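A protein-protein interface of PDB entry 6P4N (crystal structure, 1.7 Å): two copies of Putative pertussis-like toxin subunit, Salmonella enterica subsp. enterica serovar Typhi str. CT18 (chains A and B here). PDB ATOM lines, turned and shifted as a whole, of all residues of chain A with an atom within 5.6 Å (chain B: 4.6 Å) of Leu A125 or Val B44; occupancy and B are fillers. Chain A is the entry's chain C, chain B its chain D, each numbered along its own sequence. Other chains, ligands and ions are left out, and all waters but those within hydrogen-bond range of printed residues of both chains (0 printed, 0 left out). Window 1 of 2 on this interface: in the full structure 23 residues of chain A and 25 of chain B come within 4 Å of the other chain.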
ATOM      1  N   THR A  26      16.504 -14.257 -16.488  1.00  0.00           N
ATOM      2  CA  THR A  26      17.862 -13.726 -16.561  1.00  0.00           C
ATOM      3  C   THR A  26      18.915 -14.817 -16.414  1.00  0.00           C
ATOM      4  O   THR A  26      19.920 -14.823 -17.133  1.00  0.00           O
ATOM      5  CB  THR A  26      18.048 -12.673 -15.470  1.00  0.00           C
ATOM      6  OG1 THR A  26      17.143 -11.592 -15.725  1.00  0.00           O
ATOM      7  CG2 THR A  26      19.505 -12.163 -15.426  1.00  0.00           C
ATOM      8  N   ILE A  39      30.444  -0.291 -16.052  1.00  0.00           N
ATOM      9  CA  ILE A  39      29.672   0.362 -17.113  1.00  0.00           C
ATOM     10  C   ILE A  39      30.404   1.651 -17.460  1.00  0.00           C
ATOM     11  O   ILE A  39      30.491   2.566 -16.635  1.00  0.00           O
ATOM     12  CB  ILE A  39      28.224   0.638 -16.693  1.00  0.00           C
ATOM     13  CG1 ILE A  39      27.511  -0.655 -16.286  1.00  0.00           C
ATOM     14  CG2 ILE A  39      27.465   1.323 -17.840  1.00  0.00           C
ATOM     15  CD1 ILE A  39      26.061  -0.435 -15.828  1.00  0.00           C
ATOM     16  N   ILE A  55      24.369   0.221 -23.161  1.00  0.00           N
ATOM     17  CA  ILE A  55      25.527   0.428 -22.309  1.00  0.00           C
ATOM     18  C   ILE A  55      26.726  -0.276 -22.911  1.00  0.00           C
ATOM     19  O   ILE A  55      26.601  -1.277 -23.623  1.00  0.00           O
ATOM     20  CB  ILE A  55      25.295  -0.055 -20.857  1.00  0.00           C
ATOM     21  CG1 ILE A  55      24.803  -1.506 -20.813  1.00  0.00           C
ATOM     22  CG2 ILE A  55      24.312   0.882 -20.136  1.00  0.00           C
ATOM     23  CD1 ILE A  55      24.759  -2.081 -19.377  1.00  0.00           C
ATOM     24  N   GLU A  84      13.222  -0.882 -15.200  1.00  0.00           N
ATOM     25  CA  GLU A  84      14.050  -1.305 -14.071  1.00  0.00           C
ATOM     26  C   GLU A  84      15.519  -1.408 -14.465  1.00  0.00           C
ATOM     27  O   GLU A  84      16.410  -1.032 -13.691  1.00  0.00           O
ATOM     28  CB  GLU A  84      13.548  -2.646 -13.526  1.00  0.00           C
ATOM     29  CG  GLU A  84      12.276  -2.545 -12.701  1.00  0.00           C
ATOM     30  CD  GLU A  84      11.015  -2.416 -13.552  1.00  0.00           C
ATOM     31  OE1 GLU A  84      11.082  -2.529 -14.806  1.00  0.00           O
ATOM     32  OE2 GLU A  84       9.947  -2.192 -12.953  1.00  0.00           O
ATOM     33  N   LEU A  85      15.788  -1.921 -15.669  1.00  0.00           N
ATOM     34  CA  LEU A  85      17.160  -2.061 -16.133  1.00  0.00           C
ATOM     35  C   LEU A  85      17.771  -0.712 -16.476  1.00  0.00           C
ATOM     36  O   LEU A  85      18.966  -0.505 -16.254  1.00  0.00           O
ATOM     37  CB  LEU A  85      17.221  -2.977 -17.354  1.00  0.00           C
ATOM     38  CG  LEU A  85      16.894  -4.456 -17.164  1.00  0.00           C
ATOM     39  CD1 LEU A  85      16.668  -5.078 -18.541  1.00  0.00           C
ATOM     40  CD2 LEU A  85      18.010  -5.153 -16.452  1.00  0.00           C
ATOM     41  N   GLN A  88      18.656   0.785 -13.214  1.00  0.00           N
ATOM     42  CA  GLN A  88      19.781   0.133 -12.556  1.00  0.00           C
ATOM     43  C   GLN A  88      21.079   0.371 -13.309  1.00  0.00           C
ATOM     44  O   GLN A  88      22.146   0.505 -12.692  1.00  0.00           O
ATOM     45  CB  GLN A  88      19.532  -1.366 -12.402  1.00  0.00           C
ATOM     46  CG  GLN A  88      20.542  -1.978 -11.436  1.00  0.00           C
ATOM     47  CD  GLN A  88      20.399  -1.355 -10.069  1.00  0.00           C
ATOM     48  OE1 GLN A  88      19.283  -1.193  -9.580  1.00  0.00           O
ATOM     49  NE2 GLN A  88      21.525  -0.985  -9.449  1.00  0.00           N
ATOM     50  N   ALA A  89      21.016   0.413 -14.648  1.00  0.00           N
ATOM     51  CA  ALA A  89      22.197   0.760 -15.424  1.00  0.00           C
ATOM     52  C   ALA A  89      22.679   2.153 -15.054  1.00  0.00           C
ATOM     53  O   ALA A  89      23.878   2.372 -14.861  1.00  0.00           O
ATOM     54  CB  ALA A  89      21.891   0.655 -16.918  1.00  0.00           C
ATOM     55  N   PHE A  92      24.456   1.949 -11.541  1.00  0.00           N
ATOM     56  CA  PHE A  92      25.788   1.356 -11.597  1.00  0.00           C
ATOM     57  C   PHE A  92      26.744   2.184 -12.459  1.00  0.00           C
ATOM     58  O   PHE A  92      27.959   2.194 -12.216  1.00  0.00           O
ATOM     59  CB  PHE A  92      25.682  -0.075 -12.136  1.00  0.00           C
ATOM     60  CG  PHE A  92      25.146  -1.089 -11.140  1.00  0.00           C
ATOM     61  CD1 PHE A  92      25.362  -0.949  -9.769  1.00  0.00           C
ATOM     62  CD2 PHE A  92      24.452  -2.216 -11.594  1.00  0.00           C
ATOM     63  CE1 PHE A  92      24.879  -1.913  -8.870  1.00  0.00           C
ATOM     64  CE2 PHE A  92      23.973  -3.185 -10.695  1.00  0.00           C
ATOM     65  CZ  PHE A  92      24.186  -3.023  -9.337  1.00  0.00           C
ATOM     66  N   VAL A  99      30.441  -4.873 -11.779  1.00  0.00           N
ATOM     67  CA  VAL A  99      29.152  -5.531 -11.935  1.00  0.00           C
ATOM     68  C   VAL A  99      29.317  -6.758 -12.823  1.00  0.00           C
ATOM     69  O   VAL A  99      30.327  -6.933 -13.507  1.00  0.00           O
ATOM     70  CB  VAL A  99      28.077  -4.602 -12.540  1.00  0.00           C
ATOM     71  CG1 VAL A  99      27.804  -3.420 -11.612  1.00  0.00           C
ATOM     72  CG2 VAL A  99      28.522  -4.103 -13.888  1.00  0.00           C
ATOM     73  N   ARG A 100      28.294  -7.606 -12.793  1.00  0.00           N
ATOM     74  CA  ARG A 100      28.108  -8.680 -13.756  1.00  0.00           C
ATOM     75  C   ARG A 100      26.967  -8.259 -14.667  1.00  0.00           C
ATOM     76  O   ARG A 100      25.900  -7.862 -14.188  1.00  0.00           O
ATOM     77  CB  ARG A 100      27.791 -10.010 -13.061  1.00  0.00           C
ATOM     78  CG  ARG A 100      27.437 -11.128 -14.033  1.00  0.00           C
ATOM     79  CD  ARG A 100      27.183 -12.441 -13.311  1.00  0.00           C
ATOM     80  NE  ARG A 100      28.418 -12.987 -12.779  1.00  0.00           N
ATOM     81  CZ  ARG A 100      28.482 -14.099 -12.053  1.00  0.00           C
ATOM     82  NH1 ARG A 100      27.374 -14.774 -11.790  1.00  0.00           N
ATOM     83  NH2 ARG A 100      29.647 -14.533 -11.599  1.00  0.00           N
ATOM     84  N   ILE A 101      27.200  -8.309 -15.969  1.00  0.00           N
ATOM     85  CA  ILE A 101      26.198  -7.934 -16.954  1.00  0.00           C
ATOM     86  C   ILE A 101      25.705  -9.209 -17.631  1.00  0.00           C
ATOM     87  O   ILE A 101      26.512 -10.054 -18.046  1.00  0.00           O
ATOM     88  CB  ILE A 101      26.753  -6.906 -17.959  1.00  0.00           C
ATOM     89  CG1 ILE A 101      25.730  -6.603 -19.057  1.00  0.00           C
ATOM     90  CG2 ILE A 101      28.087  -7.348 -18.540  1.00  0.00           C
ATOM     91  CD1 ILE A 101      26.162  -5.493 -19.988  1.00  0.00           C
ATOM     92  N   HIS A 102      24.384  -9.373 -17.681  1.00  0.00           N
ATOM     93  CA  HIS A 102      23.727 -10.542 -18.262  1.00  0.00           C
ATOM     94  C   HIS A 102      23.065 -10.123 -19.567  1.00  0.00           C
ATOM     95  O   HIS A 102      22.358  -9.108 -19.605  1.00  0.00           O
ATOM     96  CB  HIS A 102      22.669 -11.117 -17.310  1.00  0.00           C
ATOM     97  CG  HIS A 102      23.150 -11.320 -15.905  1.00  0.00           C
ATOM     98  ND1 HIS A 102      23.440 -12.570 -15.395  1.00  0.00           N
ATOM     99  CD2 HIS A 102      23.390 -10.439 -14.903  1.00  0.00           C
ATOM    100  CE1 HIS A 102      23.834 -12.451 -14.137  1.00  0.00           C
ATOM    101  NE2 HIS A 102      23.823 -11.168 -13.815  1.00  0.00           N
ATOM    102  N   LEU A 122      20.062  -6.617 -23.115  1.00  0.00           N
ATOM    103  CA  LEU A 122      20.414  -6.591 -21.701  1.00  0.00           C
ATOM    104  C   LEU A 122      19.309  -7.260 -20.888  1.00  0.00           C
ATOM    105  O   LEU A 122      18.136  -6.885 -20.999  1.00  0.00           O
ATOM    106  CB  LEU A 122      20.619  -5.142 -21.247  1.00  0.00           C
ATOM    107  CG  LEU A 122      20.979  -4.933 -19.778  1.00  0.00           C
ATOM    108  CD1 LEU A 122      22.325  -5.554 -19.466  1.00  0.00           C
ATOM    109  CD2 LEU A 122      20.997  -3.437 -19.438  1.00  0.00           C
ATOM    110  N   VAL A 123      19.673  -8.245 -20.057  1.00  0.00           N
ATOM    111  CA  VAL A 123      18.648  -9.002 -19.342  1.00  0.00           C
ATOM    112  C   VAL A 123      18.872  -9.024 -17.831  1.00  0.00           C
ATOM    113  O   VAL A 123      18.021  -9.526 -17.081  1.00  0.00           O
ATOM    114  CB  VAL A 123      18.535 -10.440 -19.895  1.00  0.00           C
ATOM    115  CG1 VAL A 123      18.456 -10.412 -21.408  1.00  0.00           C
ATOM    116  CG2 VAL A 123      19.714 -11.314 -19.450  1.00  0.00           C
ATOM    117  N   GLY A 124      19.986  -8.471 -17.362  1.00  0.00           N
ATOM    118  CA  GLY A 124      20.156  -8.330 -15.918  1.00  0.00           C
ATOM    119  C   GLY A 124      21.455  -7.638 -15.575  1.00  0.00           C
ATOM    120  O   GLY A 124      22.372  -7.543 -16.396  1.00  0.00           O
ATOM    121  N   LEU A 125      21.516  -7.162 -14.327  1.00  0.00           N
ATOM    122  CA  LEU A 125      22.709  -6.526 -13.771  1.00  0.00           C
ATOM    123  C   LEU A 125      22.850  -6.939 -12.316  1.00  0.00           C
ATOM    124  O   LEU A 125      21.873  -6.878 -11.564  1.00  0.00           O
ATOM    125  CB  LEU A 125      22.645  -4.990 -13.857  1.00  0.00           C
ATOM    126  CG  LEU A 125      22.711  -4.391 -15.263  1.00  0.00           C
ATOM    127  CD1 LEU A 125      22.133  -2.966 -15.244  1.00  0.00           C
ATOM    128  CD2 LEU A 125      24.115  -4.390 -15.837  1.00  0.00           C
ATOM    129  N   SER A 126      24.065  -7.354 -11.926  1.00  0.00           N
ATOM    130  CA  SER A 126      24.360  -7.828 -10.575  1.00  0.00           C
ATOM    131  C   SER A 126      25.569  -7.092 -10.019  1.00  0.00           C
ATOM    132  O   SER A 126      26.552  -6.878 -10.733  1.00  0.00           O
ATOM    133  CB  SER A 126      24.668  -9.348 -10.558  1.00  0.00           C
ATOM    134  OG  SER A 126      23.692 -10.101 -11.251  1.00  0.00           O
ATOM    135  N   SER A 127      25.520  -6.732  -8.737  1.00  0.00           N
ATOM    136  CA  SER A 127      26.712  -6.182  -8.107  1.00  0.00           C
ATOM    137  C   SER A 127      27.754  -7.277  -7.900  1.00  0.00           C
ATOM    138  O   SER A 127      27.427  -8.464  -7.797  1.00  0.00           O
ATOM    139  CB  SER A 127      26.367  -5.525  -6.764  1.00  0.00           C
ATOM    140  OG  SER A 127      25.761  -6.441  -5.872  1.00  0.00           O
ATOM    141  N   LEU B  42      23.129  -6.073  -4.701  1.00  0.00           N
ATOM    142  CA  LEU B  42      21.876  -5.775  -5.390  1.00  0.00           C
ATOM    143  C   LEU B  42      21.907  -6.378  -6.787  1.00  0.00           C
ATOM    144  O   LEU B  42      22.905  -6.246  -7.502  1.00  0.00           O
ATOM    145  CB  LEU B  42      21.644  -4.256  -5.467  1.00  0.00           C
ATOM    146  CG  LEU B  42      20.444  -3.716  -6.253  1.00  0.00           C
ATOM    147  CD1 LEU B  42      19.112  -4.245  -5.721  1.00  0.00           C
ATOM    148  CD2 LEU B  42      20.482  -2.188  -6.196  1.00  0.00           C
ATOM    149  N   HIS B  43      20.810  -7.028  -7.178  1.00  0.00           N
ATOM    150  CA  HIS B  43      20.681  -7.640  -8.501  1.00  0.00           C
ATOM    151  C   HIS B  43      19.306  -7.320  -9.071  1.00  0.00           C
ATOM    152  O   HIS B  43      18.317  -7.353  -8.343  1.00  0.00           O
ATOM    153  CB  HIS B  43      20.877  -9.171  -8.405  1.00  0.00           C
ATOM    154  CG  HIS B  43      20.329  -9.934  -9.570  1.00  0.00           C
ATOM    155  ND1 HIS B  43      21.105 -10.299 -10.648  1.00  0.00           N
ATOM    156  CD2 HIS B  43      19.082 -10.403  -9.825  1.00  0.00           C
ATOM    157  CE1 HIS B  43      20.363 -10.963 -11.518  1.00  0.00           C
ATOM    158  NE2 HIS B  43      19.134 -11.043 -11.042  1.00  0.00           N
ATOM    159  N   VAL B  44      19.247  -7.006 -10.372  1.00  0.00           N
ATOM    160  CA  VAL B  44      17.993  -6.755 -11.085  1.00  0.00           C
ATOM    161  C   VAL B  44      17.916  -7.673 -12.298  1.00  0.00           C
ATOM    162  O   VAL B  44      18.895  -7.822 -13.038  1.00  0.00           O
ATOM    163  CB  VAL B  44      17.874  -5.274 -11.513  1.00  0.00           C
ATOM    164  CG1 VAL B  44      16.670  -5.053 -12.423  1.00  0.00           C
ATOM    165  CG2 VAL B  44      17.774  -4.392 -10.283  1.00  0.00           C
ATOM    166  N   GLY B  45      16.754  -8.276 -12.507  1.00  0.00           N
ATOM    167  CA  GLY B  45      16.568  -9.160 -13.634  1.00  0.00           C
ATOM    168  C   GLY B  45      15.104  -9.310 -13.983  1.00  0.00           C
ATOM    169  O   GLY B  45      14.257  -8.527 -13.542  1.00  0.00           O
ATOM    170  N   TYR B  52      12.289  -8.248 -11.442  1.00  0.00           N
ATOM    171  CA  TYR B  52      12.477  -8.589 -10.042  1.00  0.00           C
ATOM    172  C   TYR B  52      13.797  -7.990  -9.587  1.00  0.00           C
ATOM    173  O   TYR B  52      14.649  -7.621 -10.400  1.00  0.00           O
ATOM    174  CB  TYR B  52      12.441 -10.128  -9.819  1.00  0.00           C
ATOM    175  CG  TYR B  52      13.682 -10.853 -10.295  1.00  0.00           C
ATOM    176  CD1 TYR B  52      13.767 -11.354 -11.590  1.00  0.00           C
ATOM    177  CD2 TYR B  52      14.786 -11.033  -9.449  1.00  0.00           C
ATOM    178  CE1 TYR B  52      14.916 -11.998 -12.038  1.00  0.00           C
ATOM    179  CE2 TYR B  52      15.937 -11.677  -9.894  1.00  0.00           C
ATOM    180  CZ  TYR B  52      15.987 -12.161 -11.189  1.00  0.00           C
ATOM    181  OH  TYR B  52      17.126 -12.789 -11.643  1.00  0.00           O
ATOM    182  N   PHE B  53      13.967  -7.888  -8.272  1.00  0.00           N
ATOM    183  CA  PHE B  53      15.280  -7.585  -7.736  1.00  0.00           C
ATOM    184  C   PHE B  53      15.503  -8.423  -6.492  1.00  0.00           C
ATOM    185  O   PHE B  53      14.554  -8.893  -5.861  1.00  0.00           O
ATOM    186  CB  PHE B  53      15.444  -6.081  -7.433  1.00  0.00           C
ATOM    187  CG  PHE B  53      14.749  -5.614  -6.177  1.00  0.00           C
ATOM    188  CD1 PHE B  53      13.421  -5.203  -6.209  1.00  0.00           C
ATOM    189  CD2 PHE B  53      15.442  -5.526  -4.974  1.00  0.00           C
ATOM    190  CE1 PHE B  53      12.789  -4.747  -5.058  1.00  0.00           C
ATOM    191  CE2 PHE B  53      14.807  -5.070  -3.820  1.00  0.00           C
ATOM    192  CZ  PHE B  53      13.485  -4.679  -3.865  1.00  0.00           C
ATOM    193  N   ARG B  90      17.538   0.573  -2.975  1.00  0.00           N
ATOM    194  CA  ARG B  90      18.601   1.301  -3.656  1.00  0.00           C
ATOM    195  C   ARG B  90      19.182   2.394  -2.773  1.00  0.00           C
ATOM    196  O   ARG B  90      20.402   2.598  -2.751  1.00  0.00           O
ATOM    197  CB  ARG B  90      18.075   1.901  -4.963  1.00  0.00           C
ATOM    198  CG  ARG B  90      18.056   0.923  -6.109  1.00  0.00           C
ATOM    199  CD  ARG B  90      17.334   1.515  -7.304  1.00  0.00           C
ATOM    200  NE  ARG B  90      17.390   0.642  -8.469  1.00  0.00           N
ATOM    201  CZ  ARG B  90      16.458   0.620  -9.412  1.00  0.00           C
ATOM    202  NH1 ARG B  90      15.416   1.433  -9.314  1.00  0.00           N
ATOM    203  NH2 ARG B  90      16.569  -0.209 -10.444  1.00  0.00           N
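Printed residues of chain B that touch a printed residue of chain A: Leu B42, His B43, Val B44, Gly B45, Tyr B52 and Arg B90. Hydrophobic or aromatic side chains of chain B within 4 Å of the printed part of chain A: Leu B42, His B43, Val B44 and Tyr B52. Along chain B the printed residues that touch a printed residue of chain A span positions 42 to 90. Of the 18 printed residues of chain A, 9 touch a printed residue of chain B. Printed residues of chain A that touch a printed residue of chain B: Thr A26, Glu A84, Gln A88, Phe A92, Val A123, Gly A124, Leu A125, Ser A126 and Ser A127. Along chain A the printed residues that touch a printed residue of chain B span positions 26 to 127.
Thr A26 touches Gly B45 (OG1 to CA, 3.3 Å). OH of Tyr B52 touches CB of Thr A26 (3.9 Å). CD2 of Leu B42 touches NE2 of Gln A88 (3.6 Å). OE1 of Gln A88 touches CG2 of Val B44, 3.6 Å away. CZ of Phe A92 touches O of Leu B42, 3.9 Å away. CA of Gly B45 touches O of Val A123 (3.8 Å). Val B44 touches Gly A124 (O to CA, 3.2 Å). Leu A125 touches His B43. CA of Ser A126 touches O of Leu B42 (3.8 Å).
Leu A85 touches none of the printed residues of chain B. Of the printed residues of chain B, Val A123 touches Gly B45 (3.8 Å). Printed residues of chain B within 4 Å of Leu A125: His B43 and Val B44. Printed residues of chain B within 4 Å of Ser A126: Leu B42 and His B43. Of the printed residues of chain B, Ser A127 touches Leu B42 (2.9 Å). Printed residues of chain A within 4 Å of Val B44: Gln A88 (3.6 Å), Gly A124 (3.2 Å) and Leu A125 (2.9 Å). Of the printed residues of chain A, Gly B45 touches Thr A26 (3.3 Å) and Val A123 (3.8 Å). Of the printed residues of chain A, Tyr B52 touches Thr A26 (3.9 Å). Phe B53 touches none of the printed residues of chain A. The nearest printed residue of chain B that does not touch Leu A125 is Leu B42 (4.2 Å). The nearest printed residue of chain A that does not touch His B43 is His A102 (4.2 Å).
No position is printed for both chains.
O of Glu A84 sits at hydrogen-bond distance from NH2 of Arg B90, at 3.4 Å. The guanidinium group of Arg B90 lies within hydrogen-bond range of the side-chain amide oxygen of Gln A88, at 2.9 Å. The backbone carbonyl oxygen (O) of Leu A125 sits at hydrogen-bond distance from the backbone NH (N) of Val B44 (2.9 Å). A ring nitrogen (ND1) of His B43 lies within hydrogen-bond range of the side-chain hydroxyl (OG) of Ser A126 (2.7 Å). The backbone NH of Leu B42 lies within hydrogen-bond range of the side-chain hydroxyl of Ser A127, at 2.9 Å.
The side-chain hydroxyl of Thr A26 lies within hydrogen-bond range of the backbone carbonyl oxygen of Val A123, 2.6 Å away. The backbone carbonyl oxygen (O) of Ser A126 sits at hydrogen-bond distance from the backbone NH (N) of Arg A100 (2.8 Å). N of Val A123 is in hydrogen-bond range of O of His A102, 2.9 Å away. The backbone NH of His A102 lies within hydrogen-bond range of the backbone carbonyl oxygen of Gly A124, at 3.0 Å. A ring nitrogen (NE2) of His A102 lies within hydrogen-bond range of the side-chain hydroxyl of Ser A126 (2.8 Å). NE2 of His B43 lies within hydrogen-bond range of OH of Tyr B52, 2.7 Å away.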
